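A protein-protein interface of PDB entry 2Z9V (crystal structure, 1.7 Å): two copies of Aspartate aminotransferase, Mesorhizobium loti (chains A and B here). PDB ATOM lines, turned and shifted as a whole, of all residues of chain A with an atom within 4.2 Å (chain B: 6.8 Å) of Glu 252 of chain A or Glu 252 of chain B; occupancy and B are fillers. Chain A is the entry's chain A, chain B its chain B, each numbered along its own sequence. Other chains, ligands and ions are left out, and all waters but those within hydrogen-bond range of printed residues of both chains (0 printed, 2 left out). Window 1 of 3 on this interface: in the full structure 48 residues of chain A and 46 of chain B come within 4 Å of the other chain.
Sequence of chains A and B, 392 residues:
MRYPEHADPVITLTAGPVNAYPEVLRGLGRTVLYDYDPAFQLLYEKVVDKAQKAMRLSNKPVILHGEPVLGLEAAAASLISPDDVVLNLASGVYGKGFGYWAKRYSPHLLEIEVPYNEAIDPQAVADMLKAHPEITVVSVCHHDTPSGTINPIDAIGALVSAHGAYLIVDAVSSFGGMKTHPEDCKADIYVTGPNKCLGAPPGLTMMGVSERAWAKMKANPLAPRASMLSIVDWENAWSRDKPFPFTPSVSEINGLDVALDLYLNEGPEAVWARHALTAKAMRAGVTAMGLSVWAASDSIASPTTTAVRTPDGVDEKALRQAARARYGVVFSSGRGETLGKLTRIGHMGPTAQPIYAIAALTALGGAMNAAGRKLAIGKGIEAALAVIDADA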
ATOM      1  N   PRO A 201     -17.261 -23.150  16.597  1.00  0.00           N
ATOM      2  CA  PRO A 201     -18.542 -22.542  16.972  1.00  0.00           C
ATOM      3  C   PRO A 201     -19.373 -23.449  17.895  1.00  0.00           C
ATOM      4  O   PRO A 201     -19.027 -24.618  18.094  1.00  0.00           O
ATOM      5  CB  PRO A 201     -19.255 -22.367  15.617  1.00  0.00           C
ATOM      6  CG  PRO A 201     -18.691 -23.440  14.757  1.00  0.00           C
ATOM      7  CD  PRO A 201     -17.246 -23.617  15.199  1.00  0.00           C
ATOM      8  N   PRO A 202     -20.471 -22.919  18.451  1.00  0.00           N
ATOM      9  CA  PRO A 202     -21.335 -23.731  19.303  1.00  0.00           C
ATOM     10  C   PRO A 202     -22.130 -24.748  18.506  1.00  0.00           C
ATOM     11  O   PRO A 202     -22.542 -24.469  17.371  1.00  0.00           O
ATOM     12  CB  PRO A 202     -22.280 -22.698  19.934  1.00  0.00           C
ATOM     13  CG  PRO A 202     -21.692 -21.365  19.605  1.00  0.00           C
ATOM     14  CD  PRO A 202     -20.961 -21.530  18.349  1.00  0.00           C
ATOM     15  N   LEU A 204     -21.780 -28.623  19.563  1.00  0.00           N
ATOM     16  CA  LEU A 204     -21.442 -29.969  19.983  1.00  0.00           C
ATOM     17  C   LEU A 204     -21.020 -30.036  21.452  1.00  0.00           C
ATOM     18  O   LEU A 204     -20.532 -29.053  22.026  1.00  0.00           O
ATOM     19  CB  LEU A 204     -20.315 -30.534  19.120  1.00  0.00           C
ATOM     20  CG  LEU A 204     -20.642 -30.833  17.652  1.00  0.00           C
ATOM     21  CD1 LEU A 204     -19.402 -31.410  16.991  1.00  0.00           C
ATOM     22  CD2 LEU A 204     -21.862 -31.781  17.539  1.00  0.00           C
ATOM     23  N   SER A 249     -24.631 -33.682  13.592  1.00  0.00           N
ATOM     24  CA  SER A 249     -24.369 -32.377  12.981  1.00  0.00           C
ATOM     25  C   SER A 249     -23.097 -32.456  12.135  1.00  0.00           C
ATOM     26  O   SER A 249     -21.993 -32.115  12.577  1.00  0.00           O
ATOM     27  CB  SER A 249     -24.275 -31.289  14.066  1.00  0.00           C
ATOM     28  OG  SER A 249     -25.483 -31.231  14.823  1.00  0.00           O
ATOM     29  N   VAL A 250     -23.270 -32.945  10.910  1.00  0.00           N
ATOM     30  CA  VAL A 250     -22.148 -33.329  10.055  1.00  0.00           C
ATOM     31  C   VAL A 250     -21.129 -32.186   9.898  1.00  0.00           C
ATOM     32  O   VAL A 250     -19.921 -32.410  10.015  1.00  0.00           O
ATOM     33  CB  VAL A 250     -22.658 -33.815   8.674  1.00  0.00           C
ATOM     34  CG1 VAL A 250     -21.511 -34.058   7.718  1.00  0.00           C
ATOM     35  CG2 VAL A 250     -23.510 -35.101   8.851  1.00  0.00           C
ATOM     36  N   SER A 251     -21.601 -30.969   9.646  1.00  0.00           N
ATOM     37  CA  SER A 251     -20.662 -29.868   9.432  1.00  0.00           C
ATOM     38  C   SER A 251     -19.943 -29.509  10.734  1.00  0.00           C
ATOM     39  O   SER A 251     -18.749 -29.235  10.710  1.00  0.00           O
ATOM     40  CB  SER A 251     -21.303 -28.648   8.772  1.00  0.00           C
ATOM     41  OG  SER A 251     -21.760 -29.032   7.459  1.00  0.00           O
ATOM     42  N   GLU A 252     -20.655 -29.571  11.856  1.00  0.00           N
ATOM     43  CA  GLU A 252     -20.023 -29.314  13.158  1.00  0.00           C
ATOM     44  C   GLU A 252     -18.952 -30.350  13.475  1.00  0.00           C
ATOM     45  O   GLU A 252     -17.926 -30.011  14.069  1.00  0.00           O
ATOM     46  CB  GLU A 252     -21.055 -29.254  14.281  1.00  0.00           C
ATOM     47  CG  GLU A 252     -22.131 -28.193  14.097  1.00  0.00           C
ATOM     48  CD  GLU A 252     -21.594 -26.782  14.184  1.00  0.00           C
ATOM     49  OE1 GLU A 252     -20.651 -26.538  14.975  1.00  0.00           O
ATOM     50  OE2 GLU A 252     -22.122 -25.897  13.462  1.00  0.00           O
ATOM     51  N   ILE A 253     -19.181 -31.598  13.054  1.00  0.00           N
ATOM     52  CA  ILE A 253     -18.181 -32.659  13.175  1.00  0.00           C
ATOM     53  C   ILE A 253     -16.922 -32.325  12.351  1.00  0.00           C
ATOM     54  O   ILE A 253     -15.788 -32.502  12.824  1.00  0.00           O
ATOM     55  CB  ILE A 253     -18.792 -34.044  12.809  1.00  0.00           C
ATOM     56  CG1 ILE A 253     -19.752 -34.493  13.926  1.00  0.00           C
ATOM     57  CG2 ILE A 253     -17.706 -35.080  12.517  1.00  0.00           C
ATOM     58  CD1 ILE A 253     -19.060 -34.953  15.285  1.00  0.00           C
ATOM     59  N   ASN A 254     -17.130 -31.816  11.139  1.00  0.00           N
ATOM     60  CA  ASN A 254     -16.025 -31.368  10.297  1.00  0.00           C
ATOM     61  C   ASN A 254     -15.219 -30.276  11.002  1.00  0.00           C
ATOM     62  O   ASN A 254     -13.986 -30.308  11.006  1.00  0.00           O
ATOM     63  CB  ASN A 254     -16.553 -30.874   8.931  1.00  0.00           C
ATOM     64  CG  ASN A 254     -16.926 -32.020   7.981  1.00  0.00           C
ATOM     65  OD1 ASN A 254     -17.806 -31.867   7.112  1.00  0.00           O
ATOM     66  ND2 ASN A 254     -16.248 -33.142   8.108  1.00  0.00           N
ATOM     67  N   GLY A 255     -15.921 -29.333  11.626  1.00  0.00           N
ATOM     68  CA  GLY A 255     -15.258 -28.266  12.400  1.00  0.00           C
ATOM     69  C   GLY A 255     -14.491 -28.802  13.592  1.00  0.00           C
ATOM     70  O   GLY A 255     -13.366 -28.366  13.863  1.00  0.00           O
ATOM     71  N   LEU A 256     -15.103 -29.744  14.305  1.00  0.00           N
ATOM     72  CA  LEU A 256     -14.477 -30.330  15.490  1.00  0.00           C
ATOM     73  C   LEU A 256     -13.222 -31.117  15.114  1.00  0.00           C
ATOM     74  O   LEU A 256     -12.205 -31.071  15.829  1.00  0.00           O
ATOM     75  CB  LEU A 256     -15.466 -31.236  16.246  1.00  0.00           C
ATOM     76  CG  LEU A 256     -14.911 -31.979  17.470  1.00  0.00           C
ATOM     77  CD1 LEU A 256     -14.443 -31.007  18.548  1.00  0.00           C
ATOM     78  CD2 LEU A 256     -15.974 -32.912  18.034  1.00  0.00           C
ATOM     79  N   LEU B  28     -21.065 -21.355   5.815  1.00  0.00           N
ATOM     80  CA  LEU B  28     -20.701 -21.969   7.100  1.00  0.00           C
ATOM     81  C   LEU B  28     -19.359 -21.441   7.620  1.00  0.00           C
ATOM     82  O   LEU B  28     -19.084 -21.512   8.824  1.00  0.00           O
ATOM     83  CB  LEU B  28     -20.671 -23.490   6.971  1.00  0.00           C
ATOM     84  CG  LEU B  28     -22.061 -24.138   6.816  1.00  0.00           C
ATOM     85  CD1 LEU B  28     -21.941 -25.568   6.286  1.00  0.00           C
ATOM     86  CD2 LEU B  28     -22.840 -24.111   8.133  1.00  0.00           C
ATOM     87  N   HIS B  65     -32.169 -25.108  18.325  1.00  0.00           N
ATOM     88  CA  HIS B  65     -30.767 -25.358  18.024  1.00  0.00           C
ATOM     89  C   HIS B  65     -30.378 -26.813  18.162  1.00  0.00           C
ATOM     90  O   HIS B  65     -29.447 -27.191  18.893  1.00  0.00           O
ATOM     91  CB  HIS B  65     -29.902 -24.353  18.782  1.00  0.00           C
ATOM     92  CG  HIS B  65     -30.145 -22.968  18.284  1.00  0.00           C
ATOM     93  ND1 HIS B  65     -29.362 -22.386  17.312  1.00  0.00           N
ATOM     94  CD2 HIS B  65     -31.190 -22.126  18.486  1.00  0.00           C
ATOM     95  CE1 HIS B  65     -29.878 -21.209  16.988  1.00  0.00           C
ATOM     96  NE2 HIS B  65     -30.987 -21.029  17.685  1.00  0.00           N
ATOM     97  N   PRO B 194     -33.565 -27.106   7.710  1.00  0.00           N
ATOM     98  CA  PRO B 194     -32.909 -26.820   6.421  1.00  0.00           C
ATOM     99  C   PRO B 194     -32.083 -27.959   5.834  1.00  0.00           C
ATOM    100  O   PRO B 194     -31.435 -27.768   4.808  1.00  0.00           O
ATOM    101  CB  PRO B 194     -31.997 -25.637   6.759  1.00  0.00           C
ATOM    102  CG  PRO B 194     -31.583 -25.903   8.208  1.00  0.00           C
ATOM    103  CD  PRO B 194     -32.733 -26.711   8.866  1.00  0.00           C
ATOM    104  N   ALA B 200     -28.853 -27.360   3.407  1.00  0.00           N
ATOM    105  CA  ALA B 200     -27.917 -27.090   4.525  1.00  0.00           C
ATOM    106  C   ALA B 200     -27.617 -28.383   5.312  1.00  0.00           C
ATOM    107  O   ALA B 200     -28.327 -29.375   5.174  1.00  0.00           O
ATOM    108  CB  ALA B 200     -28.485 -26.020   5.457  1.00  0.00           C
ATOM    109  N   PRO B 201     -26.557 -28.381   6.147  1.00  0.00           N
ATOM    110  CA  PRO B 201     -26.312 -29.590   6.945  1.00  0.00           C
ATOM    111  C   PRO B 201     -27.289 -29.693   8.141  1.00  0.00           C
ATOM    112  O   PRO B 201     -28.038 -28.729   8.421  1.00  0.00           O
ATOM    113  CB  PRO B 201     -24.879 -29.370   7.458  1.00  0.00           C
ATOM    114  CG  PRO B 201     -24.775 -27.874   7.574  1.00  0.00           C
ATOM    115  CD  PRO B 201     -25.534 -27.346   6.375  1.00  0.00           C
ATOM    116  N   PRO B 202     -27.274 -30.840   8.854  1.00  0.00           N
ATOM    117  CA  PRO B 202     -28.131 -30.989  10.023  1.00  0.00           C
ATOM    118  C   PRO B 202     -27.685 -30.130  11.187  1.00  0.00           C
ATOM    119  O   PRO B 202     -26.475 -29.981  11.427  1.00  0.00           O
ATOM    120  CB  PRO B 202     -27.967 -32.468  10.406  1.00  0.00           C
ATOM    121  CG  PRO B 202     -27.316 -33.126   9.225  1.00  0.00           C
ATOM    122  CD  PRO B 202     -26.490 -32.066   8.587  1.00  0.00           C
ATOM    123  N   GLY B 203     -28.643 -29.570  11.918  1.00  0.00           N
ATOM    124  CA  GLY B 203     -28.276 -28.859  13.149  1.00  0.00           C
ATOM    125  C   GLY B 203     -29.316 -27.897  13.669  1.00  0.00           C
ATOM    126  O   GLY B 203     -29.276 -27.539  14.844  1.00  0.00           O
ATOM    127  N   LEU B 204     -30.244 -27.478  12.799  1.00  0.00           N
ATOM    128  CA  LEU B 204     -31.292 -26.549  13.197  1.00  0.00           C
ATOM    129  C   LEU B 204     -32.706 -27.054  12.902  1.00  0.00           C
ATOM    130  O   LEU B 204     -32.910 -27.927  12.049  1.00  0.00           O
ATOM    131  CB  LEU B 204     -31.098 -25.186  12.521  1.00  0.00           C
ATOM    132  CG  LEU B 204     -29.805 -24.418  12.818  1.00  0.00           C
ATOM    133  CD1 LEU B 204     -29.782 -23.121  12.007  1.00  0.00           C
ATOM    134  CD2 LEU B 204     -29.698 -24.129  14.314  1.00  0.00           C
ATOM    135  N   SER B 249     -26.393 -21.876  17.610  1.00  0.00           N
ATOM    136  CA  SER B 249     -25.383 -22.493  16.768  1.00  0.00           C
ATOM    137  C   SER B 249     -25.009 -21.490  15.677  1.00  0.00           C
ATOM    138  O   SER B 249     -25.546 -21.513  14.562  1.00  0.00           O
ATOM    139  CB  SER B 249     -25.904 -23.820  16.186  1.00  0.00           C
ATOM    140  OG  SER B 249     -26.248 -24.716  17.238  1.00  0.00           O
ATOM    141  N   VAL B 250     -24.076 -20.602  16.009  1.00  0.00           N
ATOM    142  CA  VAL B 250     -23.793 -19.428  15.177  1.00  0.00           C
ATOM    143  C   VAL B 250     -23.440 -19.792  13.733  1.00  0.00           C
ATOM    144  O   VAL B 250     -23.909 -19.137  12.808  1.00  0.00           O
ATOM    145  CB  VAL B 250     -22.675 -18.538  15.800  1.00  0.00           C
ATOM    146  CG1 VAL B 250     -22.286 -17.400  14.861  1.00  0.00           C
ATOM    147  CG2 VAL B 250     -23.133 -17.968  17.176  1.00  0.00           C
ATOM    148  N   SER B 251     -22.616 -20.819  13.535  1.00  0.00           N
ATOM    149  CA  SER B 251     -22.202 -21.174  12.165  1.00  0.00           C
ATOM    150  C   SER B 251     -23.363 -21.798  11.400  1.00  0.00           C
ATOM    151  O   SER B 251     -23.521 -21.540  10.204  1.00  0.00           O
ATOM    152  CB  SER B 251     -20.976 -22.082  12.160  1.00  0.00           C
ATOM    153  OG  SER B 251     -19.860 -21.370  12.684  1.00  0.00           O
ATOM    154  N   GLU B 252     -24.190 -22.578  12.094  1.00  0.00           N
ATOM    155  CA  GLU B 252     -25.398 -23.130  11.453  1.00  0.00           C
ATOM    156  C   GLU B 252     -26.347 -22.018  11.037  1.00  0.00           C
ATOM    157  O   GLU B 252     -27.013 -22.132   9.998  1.00  0.00           O
ATOM    158  CB  GLU B 252     -26.121 -24.129  12.360  1.00  0.00           C
ATOM    159  CG  GLU B 252     -25.237 -25.299  12.824  1.00  0.00           C
ATOM    160  CD  GLU B 252     -24.804 -26.200  11.682  1.00  0.00           C
ATOM    161  OE1 GLU B 252     -25.586 -26.397  10.730  1.00  0.00           O
ATOM    162  OE2 GLU B 252     -23.673 -26.715  11.721  1.00  0.00           O
ATOM    163  N   ILE B 253     -26.420 -20.955  11.839  1.00  0.00           N
ATOM    164  CA  ILE B 253     -27.254 -19.796  11.493  1.00  0.00           C
ATOM    165  C   ILE B 253     -26.711 -19.102  10.232  1.00  0.00           C
ATOM    166  O   ILE B 253     -27.482 -18.702   9.355  1.00  0.00           O
ATOM    167  CB  ILE B 253     -27.385 -18.801  12.675  1.00  0.00           C
ATOM    168  CG1 ILE B 253     -28.273 -19.391  13.790  1.00  0.00           C
ATOM    169  CG2 ILE B 253     -27.917 -17.446  12.187  1.00  0.00           C
ATOM    170  CD1 ILE B 253     -29.785 -19.529  13.430  1.00  0.00           C
ATOM    171  N   ASN B 254     -25.387 -19.019  10.114  1.00  0.00           N
ATOM    172  CA  ASN B 254     -24.767 -18.496   8.884  1.00  0.00           C
ATOM    173  C   ASN B 254     -25.152 -19.335   7.670  1.00  0.00           C
ATOM    174  O   ASN B 254     -25.461 -18.797   6.587  1.00  0.00           O
ATOM    175  CB  ASN B 254     -23.239 -18.462   9.010  1.00  0.00           C
ATOM    176  CG  ASN B 254     -22.739 -17.298   9.840  1.00  0.00           C
ATOM    177  OD1 ASN B 254     -21.699 -17.406  10.512  1.00  0.00           O
ATOM    178  ND2 ASN B 254     -23.462 -16.184   9.814  1.00  0.00           N
ATOM    179  N   GLY B 255     -25.140 -20.656   7.844  1.00  0.00           N
ATOM    180  CA  GLY B 255     -25.535 -21.584   6.776  1.00  0.00           C
ATOM    181  C   GLY B 255     -27.000 -21.420   6.408  1.00  0.00           C
ATOM    182  O   GLY B 255     -27.345 -21.390   5.229  1.00  0.00           O
ATOM    183  N   LEU B 256     -27.857 -21.308   7.423  1.00  0.00           N
ATOM    184  CA  LEU B 256     -29.301 -21.124   7.208  1.00  0.00           C
ATOM    185  C   LEU B 256     -29.601 -19.817   6.483  1.00  0.00           C
ATOM    186  O   LEU B 256     -30.449 -19.762   5.583  1.00  0.00           O
ATOM    187  CB  LEU B 256     -30.063 -21.164   8.540  1.00  0.00           C
ATOM    188  CG  LEU B 256     -31.592 -21.015   8.440  1.00  0.00           C
ATOM    189  CD1 LEU B 256     -32.242 -22.098   7.542  1.00  0.00           C
ATOM    190  CD2 LEU B 256     -32.198 -21.022   9.841  1.00  0.00           C
ATOM    191  N   ASP B 257     -28.895 -18.766   6.868  1.00  0.00           N
ATOM    192  CA  ASP B 257     -29.026 -17.462   6.235  1.00  0.00           C
ATOM    193  C   ASP B 257     -28.815 -17.590   4.720  1.00  0.00           C
ATOM    194  O   ASP B 257     -29.656 -17.147   3.919  1.00  0.00           O
ATOM    195  CB  ASP B 257     -28.006 -16.522   6.887  1.00  0.00           C
ATOM    196  CG  ASP B 257     -28.198 -15.057   6.507  1.00  0.00           C
ATOM    197  OD1 ASP B 257     -29.353 -14.588   6.348  1.00  0.00           O
ATOM    198  OD2 ASP B 257     -27.164 -14.367   6.389  1.00  0.00           O
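The side-chain carboxylate (OE2) of Glu 252 of chain A sits close to the side-chain carboxylate (OE2) of Glu 252 of chain B (2.5 Å).
ND1 of His 65 of chain B lies within hydrogen-bond range of N of Ser 249 of chain B.
OG of Ser 251 of chain B touches CG of Pro 201 of chain A (3.2 Å). Pro 202 of chain A touches Ser 249 of chain B (O to CA, 3.5 Å). CA of Ser 249 of chain A touches O of Pro 202 of chain B (3.5 Å). Ser 251 of chain A touches Leu 28 of chain B (OG to CD1, 3.7 Å). Pro 201 of chain B touches Ser 251 of chain A (CB to OG, 3.1 Å).
Glu 252 of chain A touches just one residue of chain B: Glu 252 (2.5 Å). Of chain A, only Glu 252 comes within 4 Å of Glu 252 of chain B. Printed residues of chain B within 4 Å of Pro 201 of chain A: Ser 251 (3.2 Å). Of the printed residues of chain A, Ser 251 of chain B touches Pro 201. Asn 254 of chain A touches none of the printed residues of chain B. Leu 256 of chain B touches none of the printed residues of chain A. The nearest residue of chain B that does not touch Glu 252 of chain A is Ser 251 of chain B (4.2 Å). The nearest printed residue of chain A that does not touch Glu 252 of chain B is Ser 251 of chain A (4.2 Å). The nearest printed residue of chain A that does not touch Leu 28 of chain B is Glu 252 of chain A (5.7 Å).
Printed residues of chain B that touch a printed residue of chain A: Leu 28, Pro 201, Pro 202, Ser 249, Ser 251 and Glu 252. Of the 11 printed residues of chain A, 5 touch a printed residue of chain B. Printed residues of chain A that touch a printed residue of chain B: Pro 201, Pro 202, Ser 249, Ser 251 and Glu 252. Along chain A the printed residues that touch a printed residue of chain B span positions 201 to 252. Among the printed residues, no Asp or Glu carboxylate lies within 4 Å of a Lys or Arg side-chain nitrogen of the other chain.
Pro 201 of chain A touches Ser 251 of chain B, and with the chains exchanged Ser 251 of chain A touches Pro 201 of chain B. Pro 202 of chain A touches Ser 249 of chain B, and with the chains exchanged Ser 249 of chain A touches Pro 202 of chain B. Glu 252 of chain A touches its own counterpart, Glu 252 of chain B.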
